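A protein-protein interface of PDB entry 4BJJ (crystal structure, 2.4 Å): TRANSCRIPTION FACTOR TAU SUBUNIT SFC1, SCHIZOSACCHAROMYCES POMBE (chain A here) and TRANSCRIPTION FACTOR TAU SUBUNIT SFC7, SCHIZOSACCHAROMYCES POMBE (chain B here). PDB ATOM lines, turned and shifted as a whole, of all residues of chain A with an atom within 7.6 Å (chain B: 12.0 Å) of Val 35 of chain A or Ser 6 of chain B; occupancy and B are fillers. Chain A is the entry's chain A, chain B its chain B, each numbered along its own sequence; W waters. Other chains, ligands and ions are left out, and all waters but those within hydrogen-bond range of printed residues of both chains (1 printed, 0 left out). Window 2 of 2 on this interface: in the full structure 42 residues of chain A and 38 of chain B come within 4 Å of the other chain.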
ATOM      1  N   LYS A  25     -30.454 -13.968 -28.106  1.00  0.00           N
ATOM      2  CA  LYS A  25     -29.333 -13.406 -27.357  1.00  0.00           C
ATOM      3  C   LYS A  25     -29.677 -13.081 -25.903  1.00  0.00           C
ATOM      4  O   LYS A  25     -28.943 -13.454 -24.975  1.00  0.00           O
ATOM      5  CB  LYS A  25     -28.813 -12.146 -28.051  1.00  0.00           C
ATOM      6  CG  LYS A  25     -28.063 -12.416 -29.334  1.00  0.00           C
ATOM      7  CD  LYS A  25     -27.504 -11.130 -29.937  1.00  0.00           C
ATOM      8  CE  LYS A  25     -27.205 -11.294 -31.429  1.00  0.00           C
ATOM      9  NZ  LYS A  25     -26.767 -10.026 -32.075  1.00  0.00           N
ATOM     10  N   ASP A  26     -30.796 -12.391 -25.721  1.00  0.00           N
ATOM     11  CA  ASP A  26     -31.250 -12.003 -24.400  1.00  0.00           C
ATOM     12  C   ASP A  26     -31.498 -13.223 -23.527  1.00  0.00           C
ATOM     13  O   ASP A  26     -30.973 -13.311 -22.419  1.00  0.00           O
ATOM     14  CB  ASP A  26     -32.496 -11.137 -24.519  1.00  0.00           C
ATOM     15  CG  ASP A  26     -32.232  -9.852 -25.306  1.00  0.00           C
ATOM     16  OD1 ASP A  26     -31.091  -9.336 -25.231  1.00  0.00           O
ATOM     17  OD2 ASP A  26     -33.147  -9.367 -26.014  1.00  0.00           O
ATOM     18  N   PHE A  29     -28.022 -14.877 -22.717  1.00  0.00           N
ATOM     19  CA  PHE A  29     -27.246 -14.222 -21.665  1.00  0.00           C
ATOM     20  C   PHE A  29     -27.918 -14.357 -20.317  1.00  0.00           C
ATOM     21  O   PHE A  29     -27.261 -14.419 -19.284  1.00  0.00           O
ATOM     22  CB  PHE A  29     -27.106 -12.743 -21.963  1.00  0.00           C
ATOM     23  CG  PHE A  29     -26.191 -12.445 -23.089  1.00  0.00           C
ATOM     24  CD1 PHE A  29     -24.927 -13.009 -23.136  1.00  0.00           C
ATOM     25  CD2 PHE A  29     -26.584 -11.591 -24.100  1.00  0.00           C
ATOM     26  CE1 PHE A  29     -24.077 -12.733 -24.176  1.00  0.00           C
ATOM     27  CE2 PHE A  29     -25.739 -11.309 -25.131  1.00  0.00           C
ATOM     28  CZ  PHE A  29     -24.478 -11.878 -25.170  1.00  0.00           C
ATOM     29  N   GLN A  30     -29.236 -14.387 -20.342  1.00  0.00           N
ATOM     30  CA  GLN A  30     -30.008 -14.532 -19.130  1.00  0.00           C
ATOM     31  C   GLN A  30     -29.754 -15.886 -18.444  1.00  0.00           C
ATOM     32  O   GLN A  30     -29.851 -15.985 -17.207  1.00  0.00           O
ATOM     33  CB  GLN A  30     -31.486 -14.327 -19.444  1.00  0.00           C
ATOM     34  CG  GLN A  30     -32.378 -14.261 -18.232  1.00  0.00           C
ATOM     35  CD  GLN A  30     -31.873 -13.279 -17.201  1.00  0.00           C
ATOM     36  OE1 GLN A  30     -31.401 -12.179 -17.545  1.00  0.00           O
ATOM     37  NE2 GLN A  30     -31.923 -13.689 -15.921  1.00  0.00           N
ATOM     38  N   LEU A  32     -27.132 -17.145 -17.717  1.00  0.00           N
ATOM     39  CA  LEU A  32     -25.992 -16.923 -16.832  1.00  0.00           C
ATOM     40  C   LEU A  32     -26.264 -15.742 -15.908  1.00  0.00           C
ATOM     41  O   LEU A  32     -25.389 -15.300 -15.191  1.00  0.00           O
ATOM     42  CB  LEU A  32     -24.751 -16.633 -17.657  1.00  0.00           C
ATOM     43  CG  LEU A  32     -24.276 -17.780 -18.531  1.00  0.00           C
ATOM     44  CD1 LEU A  32     -23.189 -17.306 -19.447  1.00  0.00           C
ATOM     45  CD2 LEU A  32     -23.779 -18.947 -17.684  1.00  0.00           C
ATOM     46  N   GLY A  33     -27.488 -15.233 -15.946  1.00  0.00           N
ATOM     47  CA  GLY A  33     -27.911 -14.193 -15.039  1.00  0.00           C
ATOM     48  C   GLY A  33     -27.915 -12.821 -15.664  1.00  0.00           C
ATOM     49  O   GLY A  33     -28.147 -11.831 -14.977  1.00  0.00           O
ATOM     50  N   GLY A  34     -27.649 -12.754 -16.964  1.00  0.00           N
ATOM     51  CA  GLY A  34     -27.630 -11.484 -17.680  1.00  0.00           C
ATOM     52  C   GLY A  34     -26.223 -10.980 -17.935  1.00  0.00           C
ATOM     53  O   GLY A  34     -25.259 -11.527 -17.414  1.00  0.00           O
ATOM     54  N   VAL A  35     -26.108  -9.938 -18.750  1.00  0.00           N
ATOM     55  CA  VAL A  35     -24.816  -9.443 -19.183  1.00  0.00           C
ATOM     56  C   VAL A  35     -23.997  -8.931 -18.006  1.00  0.00           C
ATOM     57  O   VAL A  35     -22.782  -9.122 -17.963  1.00  0.00           O
ATOM     58  CB  VAL A  35     -24.978  -8.333 -20.243  1.00  0.00           C
ATOM     59  CG1 VAL A  35     -23.660  -7.635 -20.518  1.00  0.00           C
ATOM     60  CG2 VAL A  35     -25.513  -8.926 -21.523  1.00  0.00           C
ATOM     61  N   GLN A  36     -24.657  -8.292 -17.047  1.00  0.00           N
ATOM     62  CA  GLN A  36     -23.936  -7.720 -15.917  1.00  0.00           C
ATOM     63  C   GLN A  36     -23.411  -8.803 -15.016  1.00  0.00           C
ATOM     64  O   GLN A  36     -22.332  -8.692 -14.473  1.00  0.00           O
ATOM     65  CB  GLN A  36     -24.808  -6.736 -15.138  1.00  0.00           C
ATOM     66  CG  GLN A  36     -24.980  -5.412 -15.883  1.00  0.00           C
ATOM     67  CD  GLN A  36     -25.886  -4.426 -15.163  1.00  0.00           C
ATOM     68  OE1 GLN A  36     -27.113  -4.528 -15.225  1.00  0.00           O
ATOM     69  NE2 GLN A  36     -25.281  -3.458 -14.484  1.00  0.00           N
ATOM     70  N   SER A  37     -24.177  -9.862 -14.870  1.00  0.00           N
ATOM     71  CA  SER A  37     -23.749 -11.001 -14.073  1.00  0.00           C
ATOM     72  C   SER A  37     -22.501 -11.672 -14.701  1.00  0.00           C
ATOM     73  O   SER A  37     -21.592 -12.118 -13.992  1.00  0.00           O
ATOM     74  CB  SER A  37     -24.909 -11.978 -13.959  1.00  0.00           C
ATOM     75  OG  SER A  37     -24.501 -13.216 -13.434  1.00  0.00           O
ATOM     76  N   ILE A  38     -22.445 -11.706 -16.032  1.00  0.00           N
ATOM     77  CA  ILE A  38     -21.303 -12.272 -16.754  1.00  0.00           C
ATOM     78  C   ILE A  38     -20.042 -11.449 -16.516  1.00  0.00           C
ATOM     79  O   ILE A  38     -18.975 -11.988 -16.251  1.00  0.00           O
ATOM     80  CB  ILE A  38     -21.618 -12.333 -18.246  1.00  0.00           C
ATOM     81  CG1 ILE A  38     -22.581 -13.486 -18.492  1.00  0.00           C
ATOM     82  CG2 ILE A  38     -20.351 -12.459 -19.098  1.00  0.00           C
ATOM     83  CD1 ILE A  38     -23.351 -13.362 -19.761  1.00  0.00           C
ATOM     84  N   GLN A  39     -20.181 -10.136 -16.595  1.00  0.00           N
ATOM     85  CA  GLN A  39     -19.074  -9.215 -16.333  1.00  0.00           C
ATOM     86  C   GLN A  39     -18.589  -9.219 -14.874  1.00  0.00           C
ATOM     87  O   GLN A  39     -17.402  -9.123 -14.592  1.00  0.00           O
ATOM     88  CB  GLN A  39     -19.484  -7.815 -16.769  1.00  0.00           C
ATOM     89  CG  GLN A  39     -19.731  -7.750 -18.268  1.00  0.00           C
ATOM     90  CD  GLN A  39     -20.348  -6.445 -18.727  1.00  0.00           C
ATOM     91  OE1 GLN A  39     -20.949  -5.705 -17.946  1.00  0.00           O
ATOM     92  NE2 GLN A  39     -20.201  -6.157 -20.011  1.00  0.00           N
ATOM     93  N   LYS A  40     -19.516  -9.355 -13.953  1.00  0.00           N
ATOM     94  CA  LYS A  40     -19.190  -9.500 -12.548  1.00  0.00           C
ATOM     95  C   LYS A  40     -18.400 -10.796 -12.348  1.00  0.00           C
ATOM     96  O   LYS A  40     -17.382 -10.806 -11.692  1.00  0.00           O
ATOM     97  CB  LYS A  40     -20.494  -9.487 -11.724  1.00  0.00           C
ATOM     98  CG  LYS A  40     -20.319  -9.304 -10.245  1.00  0.00           C
ATOM     99  CD  LYS A  40     -21.670  -9.241  -9.532  1.00  0.00           C
ATOM    100  CE  LYS A  40     -22.426 -10.582  -9.600  1.00  0.00           C
ATOM    101  NZ  LYS A  40     -23.710 -10.575  -8.832  1.00  0.00           N
ATOM    102  N   ALA A  41     -18.869 -11.888 -12.945  1.00  0.00           N
ATOM    103  CA  ALA A  41     -18.157 -13.163 -12.881  1.00  0.00           C
ATOM    104  C   ALA A  41     -16.745 -13.083 -13.472  1.00  0.00           C
ATOM    105  O   ALA A  41     -15.789 -13.561 -12.867  1.00  0.00           O
ATOM    106  CB  ALA A  41     -18.961 -14.246 -13.538  1.00  0.00           C
ATOM    107  N   SER B   6     -22.951  -4.673 -23.896  1.00  0.00           N
ATOM    108  CA  SER B   6     -23.258  -6.082 -24.082  1.00  0.00           C
ATOM    109  C   SER B   6     -22.083  -6.739 -24.757  1.00  0.00           C
ATOM    110  O   SER B   6     -20.988  -6.181 -24.788  1.00  0.00           O
ATOM    111  CB  SER B   6     -24.517  -6.270 -24.933  1.00  0.00           C
ATOM    112  OG  SER B   6     -25.580  -5.430 -24.486  1.00  0.00           O
ATOM    113  N   LEU B   7     -22.318  -7.934 -25.295  1.00  0.00           N
ATOM    114  CA  LEU B   7     -21.277  -8.710 -25.960  1.00  0.00           C
ATOM    115  C   LEU B   7     -21.693  -9.005 -27.401  1.00  0.00           C
ATOM    116  O   LEU B   7     -22.877  -9.208 -27.687  1.00  0.00           O
ATOM    117  CB  LEU B   7     -21.039 -10.020 -25.210  1.00  0.00           C
ATOM    118  CG  LEU B   7     -20.451  -9.973 -23.796  1.00  0.00           C
ATOM    119  CD1 LEU B   7     -21.347  -9.324 -22.784  1.00  0.00           C
ATOM    120  CD2 LEU B   7     -20.164 -11.369 -23.350  1.00  0.00           C
ATOM    121  N   GLU B   8     -20.702  -9.041 -28.288  1.00  0.00           N
ATOM    122  CA  GLU B   8     -20.922  -9.089 -29.736  1.00  0.00           C
ATOM    123  C   GLU B   8     -20.793 -10.488 -30.366  1.00  0.00           C
ATOM    124  O   GLU B   8     -19.801 -11.194 -30.160  1.00  0.00           O
ATOM    125  CB  GLU B   8     -19.915  -8.160 -30.422  1.00  0.00           C
ATOM    126  CG  GLU B   8     -19.851  -6.737 -29.846  1.00  0.00           C
ATOM    127  CD  GLU B   8     -18.644  -5.945 -30.359  1.00  0.00           C
ATOM    128  OE1 GLU B   8     -17.538  -6.536 -30.454  1.00  0.00           O
ATOM    129  OE2 GLU B   8     -18.803  -4.738 -30.668  1.00  0.00           O
ATOM    130  N   THR B   9     -21.790 -10.861 -31.169  1.00  0.00           N
ATOM    131  CA  THR B   9     -21.751 -12.109 -31.946  1.00  0.00           C
ATOM    132  C   THR B   9     -21.226 -11.890 -33.380  1.00  0.00           C
ATOM    133  O   THR B   9     -20.607 -10.864 -33.698  1.00  0.00           O
ATOM    134  CB  THR B   9     -23.157 -12.768 -32.033  1.00  0.00           C
ATOM    135  OG1 THR B   9     -23.922 -12.129 -33.059  1.00  0.00           O
ATOM    136  CG2 THR B   9     -23.923 -12.659 -30.700  1.00  0.00           C
ATOM    137  N   ASP B  64     -19.113 -20.253 -27.082  1.00  0.00           N
ATOM    138  CA  ASP B  64     -18.128 -19.649 -26.199  1.00  0.00           C
ATOM    139  C   ASP B  64     -18.453 -18.185 -25.979  1.00  0.00           C
ATOM    140  O   ASP B  64     -18.832 -17.475 -26.913  1.00  0.00           O
ATOM    141  CB  ASP B  64     -16.726 -19.785 -26.799  1.00  0.00           C
ATOM    142  CG  ASP B  64     -16.163 -21.189 -26.651  1.00  0.00           C
ATOM    143  OD1 ASP B  64     -16.919 -22.089 -26.215  1.00  0.00           O
ATOM    144  OD2 ASP B  64     -14.972 -21.405 -26.974  1.00  0.00           O
ATOM    145  N   ILE B  65     -18.342 -17.740 -24.734  1.00  0.00           N
ATOM    146  CA  ILE B  65     -18.336 -16.314 -24.440  1.00  0.00           C
ATOM    147  C   ILE B  65     -16.942 -15.912 -23.953  1.00  0.00           C
ATOM    148  O   ILE B  65     -16.389 -16.496 -23.029  1.00  0.00           O
ATOM    149  CB  ILE B  65     -19.397 -15.908 -23.407  1.00  0.00           C
ATOM    150  CG1 ILE B  65     -20.777 -16.348 -23.851  1.00  0.00           C
ATOM    151  CG2 ILE B  65     -19.440 -14.423 -23.256  1.00  0.00           C
ATOM    152  CD1 ILE B  65     -21.717 -16.596 -22.702  1.00  0.00           C
ATOM    153  N   VAL B  66     -16.368 -14.911 -24.606  1.00  0.00           N
ATOM    154  CA  VAL B  66     -15.039 -14.436 -24.251  1.00  0.00           C
ATOM    155  C   VAL B  66     -15.169 -13.017 -23.733  1.00  0.00           C
ATOM    156  O   VAL B  66     -15.677 -12.132 -24.409  1.00  0.00           O
ATOM    157  CB  VAL B  66     -14.062 -14.536 -25.449  1.00  0.00           C
ATOM    158  CG1 VAL B  66     -12.655 -14.594 -24.955  1.00  0.00           C
ATOM    159  CG2 VAL B  66     -14.350 -15.801 -26.252  1.00  0.00           C
ATOM    160  N   VAL B  67     -14.720 -12.815 -22.505  1.00  0.00           N
ATOM    161  CA  VAL B  67     -14.904 -11.528 -21.832  1.00  0.00           C
ATOM    162  C   VAL B  67     -13.543 -10.940 -21.466  1.00  0.00           C
ATOM    163  O   VAL B  67     -12.687 -11.633 -20.894  1.00  0.00           O
ATOM    164  CB  VAL B  67     -15.742 -11.680 -20.562  1.00  0.00           C
ATOM    165  CG1 VAL B  67     -16.057 -10.304 -19.996  1.00  0.00           C
ATOM    166  CG2 VAL B  67     -17.003 -12.454 -20.860  1.00  0.00           C
ATOM    167  N   PRO B  68     -13.332  -9.666 -21.799  1.00  0.00           N
ATOM    168  CA  PRO B  68     -12.006  -9.109 -21.517  1.00  0.00           C
ATOM    169  C   PRO B  68     -11.795  -8.697 -20.065  1.00  0.00           C
ATOM    170  O   PRO B  68     -12.700  -8.234 -19.427  1.00  0.00           O
ATOM    171  CB  PRO B  68     -11.941  -7.869 -22.426  1.00  0.00           C
ATOM    172  CG  PRO B  68     -13.336  -7.475 -22.618  1.00  0.00           C
ATOM    173  CD  PRO B  68     -14.170  -8.740 -22.578  1.00  0.00           C
ATOM    174  N   SER B  69     -10.583  -8.901 -19.589  1.00  0.00           N
ATOM    175  CA  SER B  69     -10.019  -8.165 -18.478  1.00  0.00           C
ATOM    176  C   SER B  69      -9.802  -6.696 -18.898  1.00  0.00           C
ATOM    177  O   SER B  69     -10.164  -6.298 -20.003  1.00  0.00           O
ATOM    178  CB  SER B  69      -8.690  -8.840 -18.121  1.00  0.00           C
ATOM    179  OG  SER B  69      -7.873  -8.043 -17.308  1.00  0.00           O
ATOM    180  N   GLY B  79     -16.081  -7.815 -25.444  1.00  0.00           N
ATOM    181  CA  GLY B  79     -16.961  -8.960 -25.221  1.00  0.00           C
ATOM    182  C   GLY B  79     -17.363  -9.678 -26.510  1.00  0.00           C
ATOM    183  O   GLY B  79     -17.924  -9.070 -27.412  1.00  0.00           O
ATOM    184  N   LEU B  80     -17.102 -10.982 -26.586  1.00  0.00           N
ATOM    185  CA  LEU B  80     -17.336 -11.768 -27.801  1.00  0.00           C
ATOM    186  C   LEU B  80     -18.126 -13.044 -27.576  1.00  0.00           C
ATOM    187  O   LEU B  80     -17.924 -13.763 -26.599  1.00  0.00           O
ATOM    188  CB  LEU B  80     -15.999 -12.195 -28.395  1.00  0.00           C
ATOM    189  CG  LEU B  80     -15.024 -11.077 -28.714  1.00  0.00           C
ATOM    190  CD1 LEU B  80     -13.675 -11.675 -29.028  1.00  0.00           C
ATOM    191  CD2 LEU B  80     -15.557 -10.255 -29.874  1.00  0.00           C
ATOM    192  N   VAL B  81     -18.980 -13.359 -28.535  1.00  0.00           N
ATOM    193  CA  VAL B  81     -19.744 -14.602 -28.521  1.00  0.00           C
ATOM    194  C   VAL B  81     -19.348 -15.411 -29.743  1.00  0.00           C
ATOM    195  O   VAL B  81     -19.645 -15.004 -30.864  1.00  0.00           O
ATOM    196  CB  VAL B  81     -21.254 -14.315 -28.566  1.00  0.00           C
ATOM    197  CG1 VAL B  81     -22.072 -15.602 -28.556  1.00  0.00           C
ATOM    198  CG2 VAL B  81     -21.644 -13.432 -27.416  1.00  0.00           C
ATOM    199  N   LEU B  82     -18.682 -16.547 -29.524  1.00  0.00           N
ATOM    200  CA  LEU B  82     -18.142 -17.362 -30.613  1.00  0.00           C
ATOM    201  C   LEU B  82     -18.880 -18.677 -30.731  1.00  0.00           C
ATOM    202  O   LEU B  82     -18.915 -19.471 -29.787  1.00  0.00           O
ATOM    203  CB  LEU B  82     -16.669 -17.640 -30.384  1.00  0.00           C
ATOM    204  CG  LEU B  82     -15.826 -16.404 -30.079  1.00  0.00           C
ATOM    205  CD1 LEU B  82     -14.397 -16.817 -29.797  1.00  0.00           C
ATOM    206  CD2 LEU B  82     -15.891 -15.420 -31.230  1.00  0.00           C
HETATM  207  O   HOH W   1     -24.194  -8.906 -31.170  1.00  0.00           O
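Water W1 lies within hydrogen-bond range of NZ of Lys 25 of chain A and N of Thr 9 of chain B.
CE of Lys 25 of chain A touches CG2 of Thr 9 of chain B, 3.6 Å away. Phe 29 of chain A touches Leu 7 of chain B. Val 81 of chain B touches Phe 29 of chain A (CG2 to CZ, 3.9 Å). CD1 of Leu 32 of chain A touches CD1 of Ile 65 of chain B, 3.6 Å away. Val 35 of chain A touches Ser 6 of chain B (CG1 to CA, 3.9 Å). CD1 of Leu 7 of chain B touches CG1 of Val 35 of chain A, at 3.7 Å. Ile 38 of chain A touches Val 67 of chain B (CG2 to CG2, 3.8 Å).
Phe 29 of chain A touches just these residues of chain B: Leu 7 (3.9 Å) and Val 81 (3.9 Å). No residue of chain B comes within 4 Å of Gly 34 of chain A. No residue of chain B comes within 4 Å of Gln 39 of chain A. Of the printed residues of chain A, Val 67 of chain B touches Ile 38. Of the printed residues of chain B, Lys 25 of chain A touches Thr 9 (3.6 Å). Printed residues of chain A within 4 Å of Ile 65 of chain B: Leu 32. Of the printed residues of chain A, Val 81 of chain B touches Phe 29 (3.9 Å). Asp 26 of chain A touches none of the printed residues of chain B. Glu 8 of chain B touches none of the printed residues of chain A. The nearest residue of chain B that does not touch Val 35 of chain A is Val 67 of chain B (7.1 Å). The nearest printed residue of chain A that does not touch Val 81 of chain B is Lys 25 of chain A (6.8 Å).
Along chain A the printed residues that touch a printed residue of chain B span positions 25 to 38. Hydrophobic or aromatic side chains of chain B that line the printed part of chain A: Leu 7, Ile 65, Val 67 and Val 81. Among the printed residues, 7 pairs touch across the chains. Among the printed residues, no Asp or Glu carboxylate lies within 4 Å of a Lys or Arg side-chain nitrogen of the other chain.
O of Leu 32 of chain A lies within hydrogen-bond range of OG of Ser 37 of chain A (2.9 Å). The backbone carbonyl oxygen (O) of Phe 29 of chain A sits at hydrogen-bond distance from the backbone NH (N) of Gly 34 of chain A (2.9 Å). The backbone NH (N) of Val 81 of chain B lies within hydrogen-bond range of the backbone carbonyl oxygen (O) of Glu 8 of chain B, 2.8 Å away.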
